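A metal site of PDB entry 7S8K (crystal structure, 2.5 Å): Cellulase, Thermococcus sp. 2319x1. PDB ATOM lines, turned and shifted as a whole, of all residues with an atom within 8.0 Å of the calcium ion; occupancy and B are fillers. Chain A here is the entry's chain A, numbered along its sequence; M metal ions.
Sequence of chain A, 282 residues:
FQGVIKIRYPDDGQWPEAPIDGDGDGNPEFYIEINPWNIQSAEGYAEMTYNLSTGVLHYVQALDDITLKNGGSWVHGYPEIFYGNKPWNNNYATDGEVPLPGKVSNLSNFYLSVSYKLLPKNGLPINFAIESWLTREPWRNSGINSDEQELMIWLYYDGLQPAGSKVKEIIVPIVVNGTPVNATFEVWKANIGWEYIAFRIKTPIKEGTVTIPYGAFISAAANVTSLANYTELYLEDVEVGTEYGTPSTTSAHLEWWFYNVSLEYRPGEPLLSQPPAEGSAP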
ATOM      1  N   ILE A  20       6.825  -4.734 -25.719  1.00  0.00           N
ATOM      2  CA  ILE A  20       6.840  -3.725 -26.767  1.00  0.00           C
ATOM      3  C   ILE A  20       5.382  -3.411 -27.093  1.00  0.00           C
ATOM      4  O   ILE A  20       4.671  -4.239 -27.673  1.00  0.00           O
ATOM      5  CB  ILE A  20       7.616  -4.203 -28.012  1.00  0.00           C
ATOM      6  CG1 ILE A  20       9.119  -4.031 -27.787  1.00  0.00           C
ATOM      7  CG2 ILE A  20       7.218  -3.390 -29.239  1.00  0.00           C
ATOM      8  CD1 ILE A  20       9.947  -5.138 -28.400  1.00  0.00           C
ATOM      9  N   ASP A  21       4.948  -2.216 -26.703  1.00  0.00           N
ATOM     10  CA  ASP A  21       3.553  -1.774 -26.841  1.00  0.00           C
ATOM     11  C   ASP A  21       3.568  -0.416 -27.541  1.00  0.00           C
ATOM     12  O   ASP A  21       3.462   0.623 -26.901  1.00  0.00           O
ATOM     13  CB  ASP A  21       2.869  -1.710 -25.477  1.00  0.00           C
ATOM     14  CG  ASP A  21       1.364  -1.581 -25.584  1.00  0.00           C
ATOM     15  OD1 ASP A  21       0.831  -1.720 -26.699  1.00  0.00           O
ATOM     16  OD2 ASP A  21       0.715  -1.341 -24.546  1.00  0.00           O
ATOM     17  N   GLY A  22       3.706  -0.447 -28.869  1.00  0.00           N
ATOM     18  CA  GLY A  22       3.864   0.786 -29.622  1.00  0.00           C
ATOM     19  C   GLY A  22       2.669   1.713 -29.539  1.00  0.00           C
ATOM     20  O   GLY A  22       2.826   2.935 -29.549  1.00  0.00           O
ATOM     21  N   ASP A  23       1.456   1.159 -29.470  1.00  0.00           N
ATOM     22  CA  ASP A  23       0.252   1.968 -29.419  1.00  0.00           C
ATOM     23  C   ASP A  23      -0.252   2.213 -27.998  1.00  0.00           C
ATOM     24  O   ASP A  23      -1.206   2.988 -27.827  1.00  0.00           O
ATOM     25  CB  ASP A  23      -0.872   1.312 -30.242  1.00  0.00           C
ATOM     26  CG  ASP A  23      -1.136  -0.120 -29.834  1.00  0.00           C
ATOM     27  OD1 ASP A  23      -0.536  -0.581 -28.846  1.00  0.00           O
ATOM     28  OD2 ASP A  23      -1.954  -0.786 -30.496  1.00  0.00           O
ATOM     29  N   GLY A  24       0.356   1.600 -26.991  1.00  0.00           N
ATOM     30  CA  GLY A  24      -0.033   1.845 -25.620  1.00  0.00           C
ATOM     31  C   GLY A  24      -1.424   1.387 -25.250  1.00  0.00           C
ATOM     32  O   GLY A  24      -2.057   2.005 -24.390  1.00  0.00           O
ATOM     33  N   ASP A  25      -1.908   0.319 -25.864  1.00  0.00           N
ATOM     34  CA  ASP A  25      -3.229  -0.208 -25.562  1.00  0.00           C
ATOM     35  C   ASP A  25      -3.225  -1.257 -24.456  1.00  0.00           C
ATOM     36  O   ASP A  25      -4.290  -1.764 -24.103  1.00  0.00           O
ATOM     37  CB  ASP A  25      -3.872  -0.793 -26.834  1.00  0.00           C
ATOM     38  CG  ASP A  25      -3.216  -2.082 -27.271  1.00  0.00           C
ATOM     39  OD1 ASP A  25      -2.007  -2.271 -26.998  1.00  0.00           O
ATOM     40  OD2 ASP A  25      -3.913  -2.918 -27.884  1.00  0.00           O
ATOM     41  N   GLY A  26      -2.050  -1.599 -23.928  1.00  0.00           N
ATOM     42  CA  GLY A  26      -1.931  -2.578 -22.864  1.00  0.00           C
ATOM     43  C   GLY A  26      -1.552  -3.972 -23.319  1.00  0.00           C
ATOM     44  O   GLY A  26      -1.092  -4.767 -22.500  1.00  0.00           O
ATOM     45  N   ASN A  27      -1.752  -4.284 -24.595  1.00  0.00           N
ATOM     46  CA  ASN A  27      -1.387  -5.582 -25.140  1.00  0.00           C
ATOM     47  C   ASN A  27      -0.112  -5.457 -25.939  1.00  0.00           C
ATOM     48  O   ASN A  27      -0.084  -4.686 -26.912  1.00  0.00           O
ATOM     49  CB  ASN A  27      -2.517  -6.132 -26.009  1.00  0.00           C
ATOM     50  CG  ASN A  27      -2.403  -7.633 -26.238  1.00  0.00           C
ATOM     51  OD1 ASN A  27      -1.549  -8.303 -25.659  1.00  0.00           O
ATOM     52  ND2 ASN A  27      -3.274  -8.166 -27.093  1.00  0.00           N
ATOM     53  N   PRO A  28       0.956  -6.156 -25.589  1.00  0.00           N
ATOM     54  CA  PRO A  28       2.220  -5.997 -26.323  1.00  0.00           C
ATOM     55  C   PRO A  28       2.147  -6.616 -27.711  1.00  0.00           C
ATOM     56  O   PRO A  28       1.543  -7.667 -27.915  1.00  0.00           O
ATOM     57  CB  PRO A  28       3.242  -6.714 -25.439  1.00  0.00           C
ATOM     58  CG  PRO A  28       2.547  -6.982 -24.127  1.00  0.00           C
ATOM     59  CD  PRO A  28       1.103  -7.083 -24.453  1.00  0.00           C
ATOM     60  N   GLU A  29       2.794  -5.947 -28.672  1.00  0.00           N
ATOM     61  CA  GLU A  29       3.009  -6.562 -29.974  1.00  0.00           C
ATOM     62  C   GLU A  29       4.095  -7.625 -29.898  1.00  0.00           C
ATOM     63  O   GLU A  29       4.016  -8.661 -30.575  1.00  0.00           O
ATOM     64  CB  GLU A  29       3.378  -5.500 -31.020  1.00  0.00           C
ATOM     65  CG  GLU A  29       2.357  -4.381 -31.186  1.00  0.00           C
ATOM     66  CD  GLU A  29       2.691  -3.161 -30.347  1.00  0.00           C
ATOM     67  OE1 GLU A  29       3.859  -2.719 -30.373  1.00  0.00           O
ATOM     68  OE2 GLU A  29       1.782  -2.633 -29.671  1.00  0.00           O
ATOM     69  N   PHE A  30       5.117  -7.384 -29.079  1.00  0.00           N
ATOM     70  CA  PHE A  30       6.213  -8.321 -28.912  1.00  0.00           C
ATOM     71  C   PHE A  30       6.709  -8.221 -27.479  1.00  0.00           C
ATOM     72  O   PHE A  30       6.381  -7.288 -26.746  1.00  0.00           O
ATOM     73  CB  PHE A  30       7.352  -8.046 -29.897  1.00  0.00           C
ATOM     74  CG  PHE A  30       6.959  -8.224 -31.341  1.00  0.00           C
ATOM     75  CD1 PHE A  30       6.995  -9.472 -31.934  1.00  0.00           C
ATOM     76  CD2 PHE A  30       6.559  -7.141 -32.102  1.00  0.00           C
ATOM     77  CE1 PHE A  30       6.646  -9.638 -33.263  1.00  0.00           C
ATOM     78  CE2 PHE A  30       6.199  -7.301 -33.434  1.00  0.00           C
ATOM     79  CZ  PHE A  30       6.240  -8.558 -34.008  1.00  0.00           C
ATOM     80  N   THR A  94       0.116 -10.614 -27.567  1.00  0.00           N
ATOM     81  CA  THR A  94      -0.903 -11.130 -28.474  1.00  0.00           C
ATOM     82  C   THR A  94      -1.525 -10.060 -29.359  1.00  0.00           C
ATOM     83  O   THR A  94      -2.539 -10.328 -30.016  1.00  0.00           O
ATOM     84  CB  THR A  94      -2.005 -11.856 -27.696  1.00  0.00           C
ATOM     85  OG1 THR A  94      -2.678 -10.926 -26.838  1.00  0.00           O
ATOM     86  CG2 THR A  94      -1.415 -12.989 -26.861  1.00  0.00           C
ATOM     87  N   ASP A  95      -0.965  -8.848 -29.384  1.00  0.00           N
ATOM     88  CA  ASP A  95      -1.471  -7.792 -30.268  1.00  0.00           C
ATOM     89  C   ASP A  95      -0.841  -7.984 -31.640  1.00  0.00           C
ATOM     90  O   ASP A  95       0.164  -7.369 -31.998  1.00  0.00           O
ATOM     91  CB  ASP A  95      -1.157  -6.411 -29.686  1.00  0.00           C
ATOM     92  CG  ASP A  95      -1.843  -5.293 -30.449  1.00  0.00           C
ATOM     93  OD1 ASP A  95      -2.773  -5.599 -31.224  1.00  0.00           O
ATOM     94  OD2 ASP A  95      -1.460  -4.124 -30.268  1.00  0.00           O
ATOM     95  N   GLY A  96      -1.456  -8.866 -32.431  1.00  0.00           N
ATOM     96  CA  GLY A  96      -0.897  -9.177 -33.739  1.00  0.00           C
ATOM     97  C   GLY A  96      -1.883  -9.948 -34.585  1.00  0.00           C
ATOM     98  O   GLY A  96      -2.987 -10.291 -34.154  1.00  0.00           O
HETATM   99 CA    CA M   1      -0.289  -2.975 -28.546  1.00  0.00          CA
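The calcium ion is bound by the backbone carbonyl oxygen (O) of Asn 27 (2.4 Å). The calcium ion is bound by OD2 of Asp 95 (2.4 Å). The calcium ion is bound by the side-chain carboxylate (OE2) of Glu 29, 2.4 Å away. OD1 of Asp 25 binds the calcium ion. The calcium ion is bound by OD1 of Asp 23. The side-chain carboxylate (OD1) of Asp 21 binds the calcium ion, 2.5 Å away. The calcium ion has six donor atoms within binding distance.
Of the 14 residues printed, 6 come within 4 Å of the calcium ion.
ND2 of Asn 27 lies within hydrogen-bond range of OG1 of Thr 94. N of Asp 95 lies within hydrogen-bond range of O of Pro 28 (3.1 Å). OE1 of Glu 29 lies within hydrogen-bond range of N of Gly 22, at 2.7 Å. The backbone carbonyl oxygen (O) of Ile 20 is in hydrogen-bond range of the backbone NH (N) of Glu 29, at 2.7 Å. The side-chain carboxylate (OD1) of Asp 21 lies close to the backbone NH (N) of Gly 24 (3.4 Å). OD2 of Asp 21 is in hydrogen-bond range of N of Gly 26, at 2.8 Å.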
